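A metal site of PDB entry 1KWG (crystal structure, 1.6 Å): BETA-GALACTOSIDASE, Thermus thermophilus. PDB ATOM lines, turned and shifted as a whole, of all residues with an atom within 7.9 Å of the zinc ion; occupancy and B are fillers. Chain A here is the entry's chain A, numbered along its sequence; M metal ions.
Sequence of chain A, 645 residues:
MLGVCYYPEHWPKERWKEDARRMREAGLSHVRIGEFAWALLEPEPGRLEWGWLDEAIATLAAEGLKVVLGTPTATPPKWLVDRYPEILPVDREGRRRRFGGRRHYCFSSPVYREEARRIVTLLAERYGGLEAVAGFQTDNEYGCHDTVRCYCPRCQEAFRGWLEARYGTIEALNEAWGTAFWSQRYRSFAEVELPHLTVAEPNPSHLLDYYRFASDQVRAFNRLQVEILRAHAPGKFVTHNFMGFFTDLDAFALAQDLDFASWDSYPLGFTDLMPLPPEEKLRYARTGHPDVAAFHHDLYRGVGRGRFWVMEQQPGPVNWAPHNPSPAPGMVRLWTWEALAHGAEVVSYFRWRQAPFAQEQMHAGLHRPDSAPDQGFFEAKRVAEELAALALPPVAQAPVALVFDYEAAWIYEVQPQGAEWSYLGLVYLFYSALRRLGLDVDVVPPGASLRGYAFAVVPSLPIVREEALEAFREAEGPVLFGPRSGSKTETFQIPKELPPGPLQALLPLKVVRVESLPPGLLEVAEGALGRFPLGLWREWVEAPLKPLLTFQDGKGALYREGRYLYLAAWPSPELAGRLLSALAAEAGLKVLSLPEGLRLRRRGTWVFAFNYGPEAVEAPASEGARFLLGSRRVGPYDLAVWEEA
The side-chain sulfur of Cys 150 lies close to the backbone NH of Val 90. OH of Tyr 210 lies within hydrogen-bond range of O of Cys 150 (2.7 Å). SG of Cys 152 lies close to N of Arg 154. The backbone NH (N) of Ser 108 sits close to the side-chain sulfur (SG) of Cys 106 (3.1 Å). The side-chain sulfur (SG) of Cys 106 lies close to the backbone NH (N) of Ser 109 (3.4 Å). The backbone NH of Cys 106 lies within hydrogen-bond range of the backbone carbonyl oxygen of Ile 87 (2.8 Å). The side-chain sulfur of Cys 155 sits close to the side-chain hydroxyl of Ser 108 (3.2 Å).
Four residues have an atom within 4 Å of the zinc ion: Cys 106, Cys 150, Cys 152 and Cys 155. The nearest printed residue that does not touch the zinc ion is Ser 108 (4.5 Å).
The zinc ion is bound by SG of Cys 150 (2.3 Å), SG of Cys 152 (2.4 Å), SG of Cys 106 (2.4 Å) and SG of Cys 155 (2.4 Å). The zinc ion has four donor atoms within binding distance.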
ATOM      1  N   GLU A  86      14.552  34.341   8.280  1.00  0.00           N
ATOM      2  CA  GLU A  86      14.665  32.902   8.047  1.00  0.00           C
ATOM      3  C   GLU A  86      16.058  32.364   8.330  1.00  0.00           C
ATOM      4  O   GLU A  86      16.266  31.156   8.423  1.00  0.00           O
ATOM      5  CB  GLU A  86      14.293  32.542   6.603  1.00  0.00           C
ATOM      6  CG  GLU A  86      15.310  32.965   5.545  1.00  0.00           C
ATOM      7  CD  GLU A  86      15.182  32.160   4.273  1.00  0.00           C
ATOM      8  OE1 GLU A  86      15.976  31.202   4.086  1.00  0.00           O
ATOM      9  OE2 GLU A  86      14.294  32.462   3.458  1.00  0.00           O
ATOM     10  N   ILE A  87      17.029  33.264   8.449  1.00  0.00           N
ATOM     11  CA  ILE A  87      18.411  32.851   8.740  1.00  0.00           C
ATOM     12  C   ILE A  87      18.473  32.248  10.139  1.00  0.00           C
ATOM     13  O   ILE A  87      19.230  31.297  10.375  1.00  0.00           O
ATOM     14  CB  ILE A  87      19.390  34.047   8.659  1.00  0.00           C
ATOM     15  CG1 ILE A  87      19.518  34.527   7.212  1.00  0.00           C
ATOM     16  CG2 ILE A  87      20.757  33.653   9.211  1.00  0.00           C
ATOM     17  CD1 ILE A  87      20.405  35.750   7.033  1.00  0.00           C
ATOM     18  N   LEU A  88      17.693  32.800  11.065  1.00  0.00           N
ATOM     19  CA  LEU A  88      17.677  32.319  12.446  1.00  0.00           C
ATOM     20  C   LEU A  88      17.162  30.891  12.572  1.00  0.00           C
ATOM     21  O   LEU A  88      16.126  30.540  11.999  1.00  0.00           O
ATOM     22  CB  LEU A  88      16.834  33.263  13.302  1.00  0.00           C
ATOM     23  CG  LEU A  88      17.369  34.701  13.365  1.00  0.00           C
ATOM     24  CD1 LEU A  88      16.354  35.602  14.076  1.00  0.00           C
ATOM     25  CD2 LEU A  88      18.716  34.710  14.088  1.00  0.00           C
ATOM     26  N   PRO A  89      17.867  30.049  13.338  1.00  0.00           N
ATOM     27  CA  PRO A  89      17.457  28.659  13.512  1.00  0.00           C
ATOM     28  C   PRO A  89      16.313  28.463  14.504  1.00  0.00           C
ATOM     29  O   PRO A  89      15.968  29.365  15.270  1.00  0.00           O
ATOM     30  CB  PRO A  89      18.745  27.978  13.970  1.00  0.00           C
ATOM     31  CG  PRO A  89      19.356  29.034  14.828  1.00  0.00           C
ATOM     32  CD  PRO A  89      19.145  30.310  14.027  1.00  0.00           C
ATOM     33  N   VAL A  90      15.741  27.265  14.488  1.00  0.00           N
ATOM     34  CA  VAL A  90      14.640  26.890  15.373  1.00  0.00           C
ATOM     35  C   VAL A  90      15.106  25.686  16.179  1.00  0.00           C
ATOM     36  O   VAL A  90      15.631  24.717  15.618  1.00  0.00           O
ATOM     37  CB  VAL A  90      13.382  26.517  14.566  1.00  0.00           C
ATOM     38  CG1 VAL A  90      12.312  25.958  15.487  1.00  0.00           C
ATOM     39  CG2 VAL A  90      12.856  27.749  13.835  1.00  0.00           C
ATOM     40  N   ARG A  96      12.080  29.824  17.694  1.00  0.00           N
ATOM     41  CA  ARG A  96      13.035  30.532  16.843  1.00  0.00           C
ATOM     42  C   ARG A  96      14.064  31.161  17.774  1.00  0.00           C
ATOM     43  O   ARG A  96      13.712  31.821  18.747  1.00  0.00           O
ATOM     44  CB  ARG A  96      12.309  31.613  16.042  1.00  0.00           C
ATOM     45  CG  ARG A  96      13.177  32.380  15.069  1.00  0.00           C
ATOM     46  CD  ARG A  96      13.528  31.544  13.839  1.00  0.00           C
ATOM     47  NE  ARG A  96      12.348  31.163  13.055  1.00  0.00           N
ATOM     48  CZ  ARG A  96      12.404  30.675  11.821  1.00  0.00           C
ATOM     49  NH1 ARG A  96      13.577  30.508  11.222  1.00  0.00           N
ATOM     50  NH2 ARG A  96      11.285  30.344  11.182  1.00  0.00           N
ATOM     51  N   TYR A 105      22.383  30.791  12.865  1.00  0.00           N
ATOM     52  CA  TYR A 105      21.967  30.593  11.490  1.00  0.00           C
ATOM     53  C   TYR A 105      21.628  29.150  11.200  1.00  0.00           C
ATOM     54  O   TYR A 105      22.123  28.230  11.868  1.00  0.00           O
ATOM     55  CB  TYR A 105      23.045  31.089  10.507  1.00  0.00           C
ATOM     56  CG  TYR A 105      24.299  30.251  10.395  1.00  0.00           C
ATOM     57  CD1 TYR A 105      24.330  29.082   9.633  1.00  0.00           C
ATOM     58  CD2 TYR A 105      25.475  30.658  11.032  1.00  0.00           C
ATOM     59  CE1 TYR A 105      25.501  28.348   9.495  1.00  0.00           C
ATOM     60  CE2 TYR A 105      26.645  29.927  10.910  1.00  0.00           C
ATOM     61  CZ  TYR A 105      26.658  28.768  10.140  1.00  0.00           C
ATOM     62  OH  TYR A 105      27.834  28.051  10.010  1.00  0.00           O
ATOM     63  N   CYS A 106      20.768  28.959  10.203  1.00  0.00           N
ATOM     64  CA  CYS A 106      20.324  27.647   9.768  1.00  0.00           C
ATOM     65  C   CYS A 106      21.128  27.184   8.563  1.00  0.00           C
ATOM     66  O   CYS A 106      21.290  27.925   7.587  1.00  0.00           O
ATOM     67  CB  CYS A 106      18.842  27.718   9.418  1.00  0.00           C
ATOM     68  SG  CYS A 106      18.281  26.337   8.420  1.00  0.00           S
ATOM     69  N   PHE A 107      21.631  25.953   8.626  1.00  0.00           N
ATOM     70  CA  PHE A 107      22.428  25.377   7.546  1.00  0.00           C
ATOM     71  C   PHE A 107      21.629  25.056   6.279  1.00  0.00           C
ATOM     72  O   PHE A 107      22.209  24.786   5.236  1.00  0.00           O
ATOM     73  CB  PHE A 107      23.126  24.113   8.049  1.00  0.00           C
ATOM     74  CG  PHE A 107      24.314  24.370   8.926  1.00  0.00           C
ATOM     75  CD1 PHE A 107      25.531  24.752   8.369  1.00  0.00           C
ATOM     76  CD2 PHE A 107      24.214  24.242  10.310  1.00  0.00           C
ATOM     77  CE1 PHE A 107      26.637  24.985   9.177  1.00  0.00           C
ATOM     78  CE2 PHE A 107      25.320  24.474  11.117  1.00  0.00           C
ATOM     79  CZ  PHE A 107      26.535  24.848  10.556  1.00  0.00           C
ATOM     80  N   SER A 108      20.301  25.070   6.396  1.00  0.00           N
ATOM     81  CA  SER A 108      19.438  24.778   5.250  1.00  0.00           C
ATOM     82  C   SER A 108      18.916  26.034   4.560  1.00  0.00           C
ATOM     83  O   SER A 108      18.410  25.967   3.450  1.00  0.00           O
ATOM     84  CB  SER A 108      18.229  23.936   5.688  1.00  0.00           C
ATOM     85  OG  SER A 108      18.636  22.651   6.119  1.00  0.00           O
ATOM     86  N   SER A 109      19.031  27.181   5.232  1.00  0.00           N
ATOM     87  CA  SER A 109      18.539  28.432   4.657  1.00  0.00           C
ATOM     88  C   SER A 109      19.147  28.745   3.299  1.00  0.00           C
ATOM     89  O   SER A 109      20.354  28.954   3.194  1.00  0.00           O
ATOM     90  CB  SER A 109      18.822  29.593   5.609  1.00  0.00           C
ATOM     91  OG  SER A 109      18.511  30.833   4.997  1.00  0.00           O
ATOM     92  N   THR A 147      24.044  23.564  17.280  1.00  0.00           N
ATOM     93  CA  THR A 147      23.555  24.183  16.056  1.00  0.00           C
ATOM     94  C   THR A 147      23.591  23.348  14.773  1.00  0.00           C
ATOM     95  O   THR A 147      23.313  23.863  13.692  1.00  0.00           O
ATOM     96  CB  THR A 147      24.260  25.529  15.796  1.00  0.00           C
ATOM     97  OG1 THR A 147      25.678  25.355  15.871  1.00  0.00           O
ATOM     98  CG2 THR A 147      23.821  26.556  16.839  1.00  0.00           C
ATOM     99  N   VAL A 148      23.931  22.073  14.880  1.00  0.00           N
ATOM    100  CA  VAL A 148      23.931  21.229  13.686  1.00  0.00           C
ATOM    101  C   VAL A 148      22.475  20.951  13.336  1.00  0.00           C
ATOM    102  O   VAL A 148      22.052  21.052  12.180  1.00  0.00           O
ATOM    103  CB  VAL A 148      24.650  19.871  13.914  1.00  0.00           C
ATOM    104  CG1 VAL A 148      24.394  18.935  12.730  1.00  0.00           C
ATOM    105  CG2 VAL A 148      26.146  20.095  14.088  1.00  0.00           C
ATOM    106  N   ARG A 149      21.686  20.639  14.361  1.00  0.00           N
ATOM    107  CA  ARG A 149      20.279  20.298  14.186  1.00  0.00           C
ATOM    108  C   ARG A 149      19.317  21.456  14.388  1.00  0.00           C
ATOM    109  O   ARG A 149      19.199  22.004  15.482  1.00  0.00           O
ATOM    110  CB  ARG A 149      19.944  19.138  15.117  1.00  0.00           C
ATOM    111  CG  ARG A 149      20.727  17.892  14.774  1.00  0.00           C
ATOM    112  CD  ARG A 149      21.056  17.062  15.984  1.00  0.00           C
ATOM    113  NE  ARG A 149      21.948  15.964  15.648  1.00  0.00           N
ATOM    114  CZ  ARG A 149      22.345  15.039  16.509  1.00  0.00           C
ATOM    115  NH1 ARG A 149      21.920  15.085  17.766  1.00  0.00           N
ATOM    116  NH2 ARG A 149      23.142  14.064  16.113  1.00  0.00           N
ATOM    117  N   CYS A 150      18.648  21.826  13.294  1.00  0.00           N
ATOM    118  CA  CYS A 150      17.668  22.904  13.288  1.00  0.00           C
ATOM    119  C   CYS A 150      16.332  22.298  12.884  1.00  0.00           C
ATOM    120  O   CYS A 150      16.280  21.345  12.102  1.00  0.00           O
ATOM    121  CB  CYS A 150      18.104  23.992  12.305  1.00  0.00           C
ATOM    122  SG  CYS A 150      16.886  25.308  12.055  1.00  0.00           S
ATOM    123  N   TYR A 151      15.230  22.849  13.395  1.00  0.00           N
ATOM    124  CA  TYR A 151      13.900  22.322  13.110  1.00  0.00           C
ATOM    125  C   TYR A 151      12.969  23.328  12.448  1.00  0.00           C
ATOM    126  O   TYR A 151      11.744  23.238  12.604  1.00  0.00           O
ATOM    127  CB  TYR A 151      13.287  21.819  14.414  1.00  0.00           C
ATOM    128  CG  TYR A 151      14.132  20.762  15.090  1.00  0.00           C
ATOM    129  CD1 TYR A 151      13.922  19.406  14.851  1.00  0.00           C
ATOM    130  CD2 TYR A 151      15.187  21.127  15.939  1.00  0.00           C
ATOM    131  CE1 TYR A 151      14.731  18.431  15.426  1.00  0.00           C
ATOM    132  CE2 TYR A 151      16.004  20.155  16.524  1.00  0.00           C
ATOM    133  CZ  TYR A 151      15.765  18.818  16.262  1.00  0.00           C
ATOM    134  OH  TYR A 151      16.563  17.856  16.839  1.00  0.00           O
ATOM    135  N   CYS A 152      13.546  24.270  11.715  1.00  0.00           N
ATOM    136  CA  CYS A 152      12.752  25.300  11.041  1.00  0.00           C
ATOM    137  C   CYS A 152      12.107  24.784   9.756  1.00  0.00           C
ATOM    138  O   CYS A 152      12.382  23.669   9.318  1.00  0.00           O
ATOM    139  CB  CYS A 152      13.640  26.494  10.703  1.00  0.00           C
ATOM    140  SG  CYS A 152      14.619  26.261   9.218  1.00  0.00           S
ATOM    141  N   PRO A 153      11.225  25.599   9.155  1.00  0.00           N
ATOM    142  CA  PRO A 153      10.532  25.224   7.915  1.00  0.00           C
ATOM    143  C   PRO A 153      11.483  24.884   6.772  1.00  0.00           C
ATOM    144  O   PRO A 153      11.219  23.971   5.985  1.00  0.00           O
ATOM    145  CB  PRO A 153       9.690  26.460   7.608  1.00  0.00           C
ATOM    146  CG  PRO A 153       9.346  26.958   8.970  1.00  0.00           C
ATOM    147  CD  PRO A 153      10.675  26.847   9.696  1.00  0.00           C
ATOM    148  N   ARG A 154      12.599  25.608   6.669  1.00  0.00           N
ATOM    149  CA  ARG A 154      13.575  25.354   5.621  1.00  0.00           C
ATOM    150  C   ARG A 154      14.172  23.962   5.775  1.00  0.00           C
ATOM    151  O   ARG A 154      14.407  23.262   4.789  1.00  0.00           O
ATOM    152  CB  ARG A 154      14.706  26.392   5.663  1.00  0.00           C
ATOM    153  CG  ARG A 154      14.297  27.799   5.217  1.00  0.00           C
ATOM    154  CD  ARG A 154      13.700  27.789   3.819  1.00  0.00           C
ATOM    155  NE  ARG A 154      13.606  29.136   3.262  1.00  0.00           N
ATOM    156  CZ  ARG A 154      12.940  29.444   2.152  1.00  0.00           C
ATOM    157  NH1 ARG A 154      12.295  28.504   1.481  1.00  0.00           N
ATOM    158  NH2 ARG A 154      12.922  30.700   1.719  1.00  0.00           N
ATOM    159  N   CYS A 155      14.421  23.551   7.015  1.00  0.00           N
ATOM    160  CA  CYS A 155      14.984  22.227   7.266  1.00  0.00           C
ATOM    161  C   CYS A 155      13.969  21.123   7.000  1.00  0.00           C
ATOM    162  O   CYS A 155      14.328  20.046   6.527  1.00  0.00           O
ATOM    163  CB  CYS A 155      15.503  22.126   8.703  1.00  0.00           C
ATOM    164  SG  CYS A 155      17.045  22.998   8.927  1.00  0.00           S
ATOM    165  N   GLN A 156      12.694  21.379   7.297  1.00  0.00           N
ATOM    166  CA  GLN A 156      11.673  20.373   7.045  1.00  0.00           C
ATOM    167  C   GLN A 156      11.556  20.130   5.539  1.00  0.00           C
ATOM    168  O   GLN A 156      11.433  18.990   5.102  1.00  0.00           O
ATOM    169  CB  GLN A 156      10.328  20.826   7.622  1.00  0.00           C
ATOM    170  CG  GLN A 156       9.195  19.817   7.420  1.00  0.00           C
ATOM    171  CD  GLN A 156       8.189  19.812   8.553  1.00  0.00           C
ATOM    172  OE1 GLN A 156       8.453  19.283   9.648  1.00  0.00           O
ATOM    173  NE2 GLN A 156       7.019  20.403   8.315  1.00  0.00           N
ATOM    174  N   ALA A 158      13.933  20.767   3.221  1.00  0.00           N
ATOM    175  CA  ALA A 158      15.194  20.207   2.729  1.00  0.00           C
ATOM    176  C   ALA A 158      15.318  18.726   3.091  1.00  0.00           C
ATOM    177  O   ALA A 158      15.884  17.928   2.335  1.00  0.00           O
ATOM    178  CB  ALA A 158      16.368  20.988   3.296  1.00  0.00           C
ATOM    179  N   LEU A 194       9.708  16.612  10.336  1.00  0.00           N
ATOM    180  CA  LEU A 194      10.912  16.420  11.140  1.00  0.00           C
ATOM    181  C   LEU A 194      10.519  15.586  12.359  1.00  0.00           C
ATOM    182  O   LEU A 194       9.381  15.656  12.826  1.00  0.00           O
ATOM    183  CB  LEU A 194      11.495  17.765  11.567  1.00  0.00           C
ATOM    184  CG  LEU A 194      12.008  18.645  10.420  1.00  0.00           C
ATOM    185  CD1 LEU A 194      12.564  19.934  10.983  1.00  0.00           C
ATOM    186  CD2 LEU A 194      13.068  17.915   9.608  1.00  0.00           C
ATOM    187  N   TYR A 210      17.337  11.930  10.028  1.00  0.00           N
ATOM    188  CA  TYR A 210      17.346  13.360  10.279  1.00  0.00           C
ATOM    189  C   TYR A 210      18.753  13.790  10.724  1.00  0.00           C
ATOM    190  O   TYR A 210      19.252  14.821  10.288  1.00  0.00           O
ATOM    191  CB  TYR A 210      16.315  13.747  11.344  1.00  0.00           C
ATOM    192  CG  TYR A 210      16.480  15.166  11.839  1.00  0.00           C
ATOM    193  CD1 TYR A 210      16.251  16.257  10.984  1.00  0.00           C
ATOM    194  CD2 TYR A 210      16.934  15.426  13.131  1.00  0.00           C
ATOM    195  CE1 TYR A 210      16.486  17.572  11.417  1.00  0.00           C
ATOM    196  CE2 TYR A 210      17.163  16.727  13.572  1.00  0.00           C
ATOM    197  CZ  TYR A 210      16.932  17.787  12.711  1.00  0.00           C
ATOM    198  OH  TYR A 210      17.194  19.071  13.146  1.00  0.00           O
ATOM    199  N   PHE A 213      20.999  13.732   7.754  1.00  0.00           N
ATOM    200  CA  PHE A 213      20.641  14.909   6.964  1.00  0.00           C
ATOM    201  C   PHE A 213      21.268  16.180   7.522  1.00  0.00           C
ATOM    202  O   PHE A 213      21.867  16.965   6.794  1.00  0.00           O
ATOM    203  CB  PHE A 213      19.112  15.054   6.921  1.00  0.00           C
ATOM    204  CG  PHE A 213      18.643  16.452   6.652  1.00  0.00           C
ATOM    205  CD1 PHE A 213      18.723  17.009   5.387  1.00  0.00           C
ATOM    206  CD2 PHE A 213      18.112  17.224   7.688  1.00  0.00           C
ATOM    207  CE1 PHE A 213      18.289  18.316   5.145  1.00  0.00           C
ATOM    208  CE2 PHE A 213      17.679  18.521   7.466  1.00  0.00           C
ATOM    209  CZ  PHE A 213      17.760  19.074   6.184  1.00  0.00           C
ATOM    210  N   GLN A 217      23.938  18.630   5.731  1.00  0.00           N
ATOM    211  CA  GLN A 217      23.698  20.045   5.408  1.00  0.00           C
ATOM    212  C   GLN A 217      24.902  20.884   5.810  1.00  0.00           C
ATOM    213  O   GLN A 217      25.245  21.858   5.126  1.00  0.00           O
ATOM    214  CB  GLN A 217      22.442  20.560   6.117  1.00  0.00           C
ATOM    215  CG  GLN A 217      21.130  20.023   5.575  1.00  0.00           C
ATOM    216  CD  GLN A 217      20.877  20.447   4.137  1.00  0.00           C
ATOM    217  OE1 GLN A 217      21.540  19.988   3.203  1.00  0.00           O
ATOM    218  NE2 GLN A 217      19.904  21.332   3.954  1.00  0.00           N
HETATM  219 ZN    ZN M   1      16.666  25.219   9.718  1.00  0.00          ZN
